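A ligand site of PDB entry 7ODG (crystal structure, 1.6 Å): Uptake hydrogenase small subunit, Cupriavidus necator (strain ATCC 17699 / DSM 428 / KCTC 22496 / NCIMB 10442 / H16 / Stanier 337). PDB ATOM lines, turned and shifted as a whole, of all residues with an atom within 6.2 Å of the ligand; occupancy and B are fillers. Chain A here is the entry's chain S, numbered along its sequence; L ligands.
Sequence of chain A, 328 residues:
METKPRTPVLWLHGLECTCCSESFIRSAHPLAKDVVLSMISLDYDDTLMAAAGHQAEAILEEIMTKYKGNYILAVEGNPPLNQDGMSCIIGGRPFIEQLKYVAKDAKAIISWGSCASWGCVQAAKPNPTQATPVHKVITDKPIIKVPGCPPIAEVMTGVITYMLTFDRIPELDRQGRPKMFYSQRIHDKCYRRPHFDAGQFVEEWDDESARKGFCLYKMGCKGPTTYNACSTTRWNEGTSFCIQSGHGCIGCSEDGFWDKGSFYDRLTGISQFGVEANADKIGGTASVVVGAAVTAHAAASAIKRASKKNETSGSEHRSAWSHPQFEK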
ATOM      1  N   ILE A 186     -31.143  -5.631   2.038  1.00  0.00           N
ATOM      2  CA  ILE A 186     -31.356  -7.061   2.071  1.00  0.00           C
ATOM      3  C   ILE A 186     -31.230  -7.547   3.509  1.00  0.00           C
ATOM      4  O   ILE A 186     -32.036  -8.339   3.982  1.00  0.00           O
ATOM      5  CB  ILE A 186     -30.320  -7.804   1.181  1.00  0.00           C
ATOM      6  CG1 ILE A 186     -30.431  -7.382  -0.289  1.00  0.00           C
ATOM      7  CG2 ILE A 186     -30.421  -9.313   1.348  1.00  0.00           C
ATOM      8  CD1 ILE A 186     -31.754  -7.680  -0.940  1.00  0.00           C
ATOM      9  N   HIS A 187     -30.201  -7.073   4.189  1.00  0.00           N
ATOM     10  CA  HIS A 187     -29.879  -7.482   5.581  1.00  0.00           C
ATOM     11  C   HIS A 187     -30.954  -7.110   6.635  1.00  0.00           C
ATOM     12  O   HIS A 187     -31.007  -7.725   7.701  1.00  0.00           O
ATOM     13  CB  HIS A 187     -28.518  -6.846   5.909  1.00  0.00           C
ATOM     14  CG  HIS A 187     -27.948  -7.183   7.247  1.00  0.00           C
ATOM     15  ND1 HIS A 187     -27.445  -8.427   7.551  1.00  0.00           N
ATOM     16  CD2 HIS A 187     -27.696  -6.413   8.333  1.00  0.00           C
ATOM     17  CE1 HIS A 187     -26.956  -8.427   8.777  1.00  0.00           C
ATOM     18  NE2 HIS A 187     -27.096  -7.217   9.279  1.00  0.00           N
ATOM     19  N   ASP A 188     -31.802  -6.117   6.340  1.00  0.00           N
ATOM     20  CA  ASP A 188     -32.859  -5.700   7.283  1.00  0.00           C
ATOM     21  C   ASP A 188     -33.838  -6.828   7.649  1.00  0.00           C
ATOM     22  O   ASP A 188     -34.094  -7.044   8.828  1.00  0.00           O
ATOM     23  CB  ASP A 188     -33.659  -4.493   6.742  1.00  0.00           C
ATOM     24  CG  ASP A 188     -32.822  -3.221   6.571  1.00  0.00           C
ATOM     25  OD1 ASP A 188     -31.715  -3.130   7.176  1.00  0.00           O
ATOM     26  OD2 ASP A 188     -33.264  -2.288   5.846  1.00  0.00           O
ATOM     27  N   CYS A 190     -33.679 -10.131   5.966  1.00  0.00           N
ATOM     28  CA  CYS A 190     -33.137 -11.429   5.612  1.00  0.00           C
ATOM     29  C   CYS A 190     -33.458 -12.472   6.707  1.00  0.00           C
ATOM     30  O   CYS A 190     -33.199 -12.243   7.902  1.00  0.00           O
ATOM     31  CB  CYS A 190     -31.624 -11.345   5.395  1.00  0.00           C
ATOM     32  SG  CYS A 190     -30.819 -12.922   5.062  1.00  0.00           S
ATOM     33  N   TYR A 191     -34.014 -13.612   6.299  1.00  0.00           N
ATOM     34  CA  TYR A 191     -34.429 -14.654   7.244  1.00  0.00           C
ATOM     35  C   TYR A 191     -33.257 -15.290   8.022  1.00  0.00           C
ATOM     36  O   TYR A 191     -33.494 -15.997   9.019  1.00  0.00           O
ATOM     37  CB  TYR A 191     -35.272 -15.732   6.542  1.00  0.00           C
ATOM     38  CG  TYR A 191     -34.453 -16.765   5.807  1.00  0.00           C
ATOM     39  CD1 TYR A 191     -33.864 -16.483   4.585  1.00  0.00           C
ATOM     40  CD2 TYR A 191     -34.246 -18.027   6.354  1.00  0.00           C
ATOM     41  CE1 TYR A 191     -33.093 -17.421   3.941  1.00  0.00           C
ATOM     42  CE2 TYR A 191     -33.476 -18.979   5.704  1.00  0.00           C
ATOM     43  CZ  TYR A 191     -32.911 -18.651   4.482  1.00  0.00           C
ATOM     44  OH  TYR A 191     -32.125 -19.560   3.821  1.00  0.00           O
ATOM     45  N   ARG A 192     -32.017 -15.086   7.572  1.00  0.00           N
ATOM     46  CA  ARG A 192     -30.838 -15.611   8.285  1.00  0.00           C
ATOM     47  C   ARG A 192     -30.350 -14.650   9.361  1.00  0.00           C
ATOM     48  O   ARG A 192     -29.381 -14.974  10.071  1.00  0.00           O
ATOM     49  CB  ARG A 192     -29.713 -15.931   7.289  1.00  0.00           C
ATOM     50  CG  ARG A 192     -30.077 -17.006   6.282  1.00  0.00           C
ATOM     51  CD  ARG A 192     -28.876 -17.673   5.649  1.00  0.00           C
ATOM     52  NE  ARG A 192     -29.300 -18.655   4.662  1.00  0.00           N
ATOM     53  CZ  ARG A 192     -28.552 -19.666   4.194  1.00  0.00           C
ATOM     54  NH1 ARG A 192     -27.302 -19.852   4.595  1.00  0.00           N
ATOM     55  NH2 ARG A 192     -29.062 -20.494   3.299  1.00  0.00           N
ATOM     56  N   ARG A 193     -30.985 -13.491   9.497  1.00  0.00           N
ATOM     57  CA  ARG A 193     -30.579 -12.488  10.510  1.00  0.00           C
ATOM     58  C   ARG A 193     -30.380 -12.988  11.941  1.00  0.00           C
ATOM     59  O   ARG A 193     -29.439 -12.564  12.598  1.00  0.00           O
ATOM     60  CB  ARG A 193     -31.546 -11.294  10.551  1.00  0.00           C
ATOM     61  CG  ARG A 193     -31.134 -10.115   9.683  1.00  0.00           C
ATOM     62  CD  ARG A 193     -29.770  -9.522  10.040  1.00  0.00           C
ATOM     63  NE  ARG A 193     -29.738  -8.802  11.310  1.00  0.00           N
ATOM     64  CZ  ARG A 193     -30.173  -7.562  11.504  1.00  0.00           C
ATOM     65  NH1 ARG A 193     -30.708  -6.869  10.510  1.00  0.00           N
ATOM     66  NH2 ARG A 193     -30.063  -7.007  12.708  1.00  0.00           N
ATOM     67  N   PRO A 194     -31.280 -13.856  12.435  1.00  0.00           N
ATOM     68  CA  PRO A 194     -31.093 -14.396  13.779  1.00  0.00           C
ATOM     69  C   PRO A 194     -29.772 -15.144  13.964  1.00  0.00           C
ATOM     70  O   PRO A 194     -29.220 -15.136  15.055  1.00  0.00           O
ATOM     71  CB  PRO A 194     -32.292 -15.343  13.931  1.00  0.00           C
ATOM     72  CG  PRO A 194     -33.346 -14.685  13.096  1.00  0.00           C
ATOM     73  CD  PRO A 194     -32.592 -14.238  11.877  1.00  0.00           C
ATOM     74  N   PHE A 196     -26.973 -14.262  12.041  1.00  0.00           N
ATOM     75  CA  PHE A 196     -26.043 -13.134  12.052  1.00  0.00           C
ATOM     76  C   PHE A 196     -25.962 -12.537  13.454  1.00  0.00           C
ATOM     77  O   PHE A 196     -24.879 -12.303  13.953  1.00  0.00           O
ATOM     78  CB  PHE A 196     -26.456 -12.032  11.079  1.00  0.00           C
ATOM     79  CG  PHE A 196     -25.549 -10.818  11.106  1.00  0.00           C
ATOM     80  CD1 PHE A 196     -24.418 -10.746  10.292  1.00  0.00           C
ATOM     81  CD2 PHE A 196     -25.848  -9.727  11.927  1.00  0.00           C
ATOM     82  CE1 PHE A 196     -23.600  -9.627  10.311  1.00  0.00           C
ATOM     83  CE2 PHE A 196     -25.030  -8.608  11.945  1.00  0.00           C
ATOM     84  CZ  PHE A 196     -23.904  -8.557  11.144  1.00  0.00           C
ATOM     85  N   PHE A 201     -22.208 -18.444  11.570  1.00  0.00           N
ATOM     86  CA  PHE A 201     -21.797 -18.196  10.193  1.00  0.00           C
ATOM     87  C   PHE A 201     -21.358 -19.456   9.467  1.00  0.00           C
ATOM     88  O   PHE A 201     -20.840 -20.401  10.087  1.00  0.00           O
ATOM     89  CB  PHE A 201     -20.632 -17.202  10.172  1.00  0.00           C
ATOM     90  CG  PHE A 201     -20.944 -15.883  10.824  1.00  0.00           C
ATOM     91  CD1 PHE A 201     -21.782 -14.974  10.208  1.00  0.00           C
ATOM     92  CD2 PHE A 201     -20.374 -15.549  12.051  1.00  0.00           C
ATOM     93  CE1 PHE A 201     -22.077 -13.754  10.803  1.00  0.00           C
ATOM     94  CE2 PHE A 201     -20.655 -14.331  12.649  1.00  0.00           C
ATOM     95  CZ  PHE A 201     -21.506 -13.433  12.025  1.00  0.00           C
ATOM     96  N   PHE A 214     -26.996 -21.138   8.242  1.00  0.00           N
ATOM     97  CA  PHE A 214     -26.342 -20.046   8.972  1.00  0.00           C
ATOM     98  C   PHE A 214     -26.015 -18.868   8.034  1.00  0.00           C
ATOM     99  O   PHE A 214     -26.062 -18.992   6.798  1.00  0.00           O
ATOM    100  CB  PHE A 214     -25.068 -20.550   9.666  1.00  0.00           C
ATOM    101  CG  PHE A 214     -25.309 -21.313  10.952  1.00  0.00           C
ATOM    102  CD1 PHE A 214     -26.580 -21.756  11.331  1.00  0.00           C
ATOM    103  CD2 PHE A 214     -24.233 -21.620  11.768  1.00  0.00           C
ATOM    104  CE1 PHE A 214     -26.756 -22.460  12.526  1.00  0.00           C
ATOM    105  CE2 PHE A 214     -24.406 -22.321  12.954  1.00  0.00           C
ATOM    106  CZ  PHE A 214     -25.672 -22.743  13.320  1.00  0.00           C
ATOM    107  N   CYS A 215     -25.702 -17.733   8.649  1.00  0.00           N
ATOM    108  CA  CYS A 215     -25.510 -16.477   7.937  1.00  0.00           C
ATOM    109  C   CYS A 215     -24.305 -16.566   6.991  1.00  0.00           C
ATOM    110  O   CYS A 215     -23.303 -17.230   7.317  1.00  0.00           O
ATOM    111  CB  CYS A 215     -25.327 -15.324   8.945  1.00  0.00           C
ATOM    112  SG  CYS A 215     -24.808 -13.764   8.206  1.00  0.00           S
ATOM    113  N   LEU A 216     -24.423 -15.919   5.832  1.00  0.00           N
ATOM    114  CA  LEU A 216     -23.398 -15.941   4.782  1.00  0.00           C
ATOM    115  C   LEU A 216     -22.431 -14.747   4.762  1.00  0.00           C
ATOM    116  O   LEU A 216     -21.636 -14.597   3.804  1.00  0.00           O
ATOM    117  CB  LEU A 216     -24.067 -16.112   3.402  1.00  0.00           C
ATOM    118  CG  LEU A 216     -24.912 -17.402   3.240  1.00  0.00           C
ATOM    119  CD1 LEU A 216     -25.870 -17.375   2.056  1.00  0.00           C
ATOM    120  CD2 LEU A 216     -24.015 -18.626   3.143  1.00  0.00           C
ATOM    121  N   TYR A 217     -22.455 -13.924   5.801  1.00  0.00           N
ATOM    122  CA  TYR A 217     -21.546 -12.771   5.882  1.00  0.00           C
ATOM    123  C   TYR A 217     -20.073 -13.131   5.653  1.00  0.00           C
ATOM    124  O   TYR A 217     -19.365 -12.448   4.906  1.00  0.00           O
ATOM    125  CB  TYR A 217     -21.679 -12.107   7.260  1.00  0.00           C
ATOM    126  CG  TYR A 217     -20.925 -10.805   7.412  1.00  0.00           C
ATOM    127  CD1 TYR A 217     -19.613 -10.774   7.840  1.00  0.00           C
ATOM    128  CD2 TYR A 217     -21.544  -9.592   7.150  1.00  0.00           C
ATOM    129  CE1 TYR A 217     -18.939  -9.575   8.005  1.00  0.00           C
ATOM    130  CE2 TYR A 217     -20.887  -8.395   7.321  1.00  0.00           C
ATOM    131  CZ  TYR A 217     -19.582  -8.383   7.739  1.00  0.00           C
ATOM    132  OH  TYR A 217     -18.924  -7.194   7.873  1.00  0.00           O
ATOM    133  N   CYS A 221     -21.223 -12.234   1.748  1.00  0.00           N
ATOM    134  CA  CYS A 221     -22.566 -11.667   1.540  1.00  0.00           C
ATOM    135  C   CYS A 221     -22.589 -10.136   1.680  1.00  0.00           C
ATOM    136  O   CYS A 221     -22.166  -9.580   2.686  1.00  0.00           O
ATOM    137  CB  CYS A 221     -23.619 -12.309   2.460  1.00  0.00           C
ATOM    138  SG  CYS A 221     -25.289 -11.640   2.198  1.00  0.00           S
ATOM    139  N   LYS A 222     -23.056  -9.484   0.634  1.00  0.00           N
ATOM    140  CA  LYS A 222     -23.120  -8.032   0.574  1.00  0.00           C
ATOM    141  C   LYS A 222     -24.513  -7.486   0.890  1.00  0.00           C
ATOM    142  O   LYS A 222     -24.748  -6.299   0.719  1.00  0.00           O
ATOM    143  CB  LYS A 222     -22.609  -7.542  -0.799  1.00  0.00           C
ATOM    144  CG  LYS A 222     -21.162  -7.942  -1.119  1.00  0.00           C
ATOM    145  CD  LYS A 222     -20.228  -7.634   0.048  1.00  0.00           C
ATOM    146  CE  LYS A 222     -18.754  -7.818  -0.278  1.00  0.00           C
ATOM    147  NZ  LYS A 222     -18.438  -9.122  -0.911  1.00  0.00           N
ATOM    148  N   GLY A 223     -25.387  -8.336   1.433  1.00  0.00           N
ATOM    149  CA  GLY A 223     -26.704  -7.890   1.898  1.00  0.00           C
ATOM    150  C   GLY A 223     -26.715  -6.706   2.874  1.00  0.00           C
ATOM    151  O   GLY A 223     -27.592  -5.864   2.801  1.00  0.00           O
ATOM    152  N   PRO A 224     -25.724  -6.609   3.771  1.00  0.00           N
ATOM    153  CA  PRO A 224     -25.663  -5.446   4.681  1.00  0.00           C
ATOM    154  C   PRO A 224     -25.502  -4.076   4.028  1.00  0.00           C
ATOM    155  O   PRO A 224     -25.764  -3.081   4.687  1.00  0.00           O
ATOM    156  CB  PRO A 224     -24.470  -5.765   5.581  1.00  0.00           C
ATOM    157  CG  PRO A 224     -24.420  -7.250   5.590  1.00  0.00           C
ATOM    158  CD  PRO A 224     -24.753  -7.641   4.175  1.00  0.00           C
ATOM    159  N   SER A 231     -35.256 -10.010  -0.073  1.00  0.00           N
ATOM    160  CA  SER A 231     -35.470 -10.744   1.177  1.00  0.00           C
ATOM    161  C   SER A 231     -36.942 -10.944   1.528  1.00  0.00           C
ATOM    162  O   SER A 231     -37.312 -11.921   2.199  1.00  0.00           O
ATOM    163  CB  SER A 231     -34.800 -10.011   2.360  1.00  0.00           C
ATOM    164  OG  SER A 231     -33.407  -9.980   2.220  1.00  0.00           O
ATOM    165  N   PHE A 241     -34.484 -16.512  -3.032  1.00  0.00           N
ATOM    166  CA  PHE A 241     -33.544 -15.487  -3.406  1.00  0.00           C
ATOM    167  C   PHE A 241     -32.145 -15.994  -3.159  1.00  0.00           C
ATOM    168  O   PHE A 241     -31.962 -17.121  -2.665  1.00  0.00           O
ATOM    169  CB  PHE A 241     -33.844 -14.133  -2.726  1.00  0.00           C
ATOM    170  CG  PHE A 241     -33.571 -14.079  -1.252  1.00  0.00           C
ATOM    171  CD1 PHE A 241     -34.289 -14.873  -0.363  1.00  0.00           C
ATOM    172  CD2 PHE A 241     -32.683 -13.139  -0.738  1.00  0.00           C
ATOM    173  CE1 PHE A 241     -34.085 -14.759   1.004  1.00  0.00           C
ATOM    174  CE2 PHE A 241     -32.465 -13.026   0.633  1.00  0.00           C
ATOM    175  CZ  PHE A 241     -33.168 -13.845   1.506  1.00  0.00           C
ATOM    176  N   ILE A 243     -29.730 -15.698  -1.107  1.00  0.00           N
ATOM    177  CA  ILE A 243     -29.351 -16.170   0.231  1.00  0.00           C
ATOM    178  C   ILE A 243     -30.114 -17.432   0.640  1.00  0.00           C
ATOM    179  O   ILE A 243     -29.531 -18.369   1.237  1.00  0.00           O
ATOM    180  CB  ILE A 243     -29.506 -15.014   1.243  1.00  0.00           C
ATOM    181  CG1 ILE A 243     -28.386 -13.990   0.998  1.00  0.00           C
ATOM    182  CG2 ILE A 243     -29.500 -15.489   2.695  1.00  0.00           C
ATOM    183  CD1 ILE A 243     -28.752 -12.571   1.350  1.00  0.00           C
ATOM    184  N   GLY A 248     -24.250 -15.947  -0.928  1.00  0.00           N
ATOM    185  CA  GLY A 248     -24.319 -14.558  -0.457  1.00  0.00           C
ATOM    186  C   GLY A 248     -24.799 -13.610  -1.555  1.00  0.00           C
ATOM    187  O   GLY A 248     -24.653 -13.889  -2.753  1.00  0.00           O
ATOM    188  N   CYS A 249     -25.453 -12.519  -1.139  1.00  0.00           N
ATOM    189  CA  CYS A 249     -25.787 -11.435  -2.051  1.00  0.00           C
ATOM    190  C   CYS A 249     -24.475 -10.876  -2.605  1.00  0.00           C
ATOM    191  O   CYS A 249     -23.521 -10.674  -1.833  1.00  0.00           O
ATOM    192  CB  CYS A 249     -26.553 -10.346  -1.268  1.00  0.00           C
ATOM    193  SG  CYS A 249     -26.847  -8.784  -2.098  1.00  0.00           S
HETATM  194 FE1  LIG L   1     -28.684 -12.391   5.473  1.00  0.00          FE
HETATM  195 FE2  LIG L   1     -26.325 -11.778   4.264  1.00  0.00          FE
HETATM  196 FE3  LIG L   1     -26.313 -12.792   6.818  1.00  0.00          FE
HETATM  197 FE4  LIG L   1     -27.227 -10.300   6.404  1.00  0.00          FE
HETATM  198  S1  LIG L   1     -28.236 -11.914   7.649  1.00  0.00           S
HETATM  199  S2  LIG L   1     -25.055 -11.031   5.995  1.00  0.00           S
HETATM  200  S3  LIG L   1     -27.002 -13.873   4.954  1.00  0.00           S
HETATM  201  S4  LIG L   1     -28.181 -10.491   4.330  1.00  0.00           S
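An iron atom (FE4) of the ligand is bound by a ring nitrogen (ND1) of His 187 (2.2 Å).
An iron atom (FE1) of the ligand is bound by the side-chain sulfur (SG) of Cys 190.
An iron atom (FE3) of the ligand is bound by the side-chain sulfur (SG) of Cys 215 (2.3 Å).
The side-chain sulfur of Cys 221 binds an iron atom (FE2) of the ligand.
S3 of the ligand lies close to N of Leu 216.
N of Arg 193 lies close to S1 of the ligand.
O of His 187 is in hydrogen-bond range of NH1 of Arg 193, 3.0 Å away.
O of Gly 223 is in hydrogen-bond range of N of His 187.
N of Arg 192 lies close to SG of Cys 190 (3.5 Å).
The side-chain sulfur (SG) of Cys 221 lies close to the backbone NH (N) of Gly 223 (3.4 Å).
The backbone NH (N) of Cys 249 sits close to the side-chain sulfur (SG) of Cys 221.
NH2 of Arg 192 sits at hydrogen-bond distance from O of Ile 243 (3.0 Å).
The guanidinium group of Arg 192 sits at hydrogen-bond distance from the backbone carbonyl oxygen of Phe 214.
The backbone carbonyl oxygen of Ile 186 is in hydrogen-bond range of the side-chain hydroxyl of Ser 231.
Ile 186 touches the ligand (CG2 to S4, 3.9 Å).
C of Arg 192 touches S1 of the ligand, 3.9 Å away.
Phe 196 touches the ligand.
Tyr 217 touches the ligand (CB to S2, 3.8 Å).
Gly 223 touches the ligand.
Pro 224 touches the ligand.
Ile 243 touches the ligand.
Hydrophobic or aromatic side chains within 4 Å of the ligand: Ile 186, His 187, Phe 196, Tyr 217, Pro 224 and Ile 243.
13 residues have an atom within 4 Å of the ligand: Ile 186, His 187, Cys 190, Arg 192, Arg 193, Phe 196, Cys 215, Leu 216, Tyr 217, Cys 221, Gly 223, Pro 224 and Ile 243.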
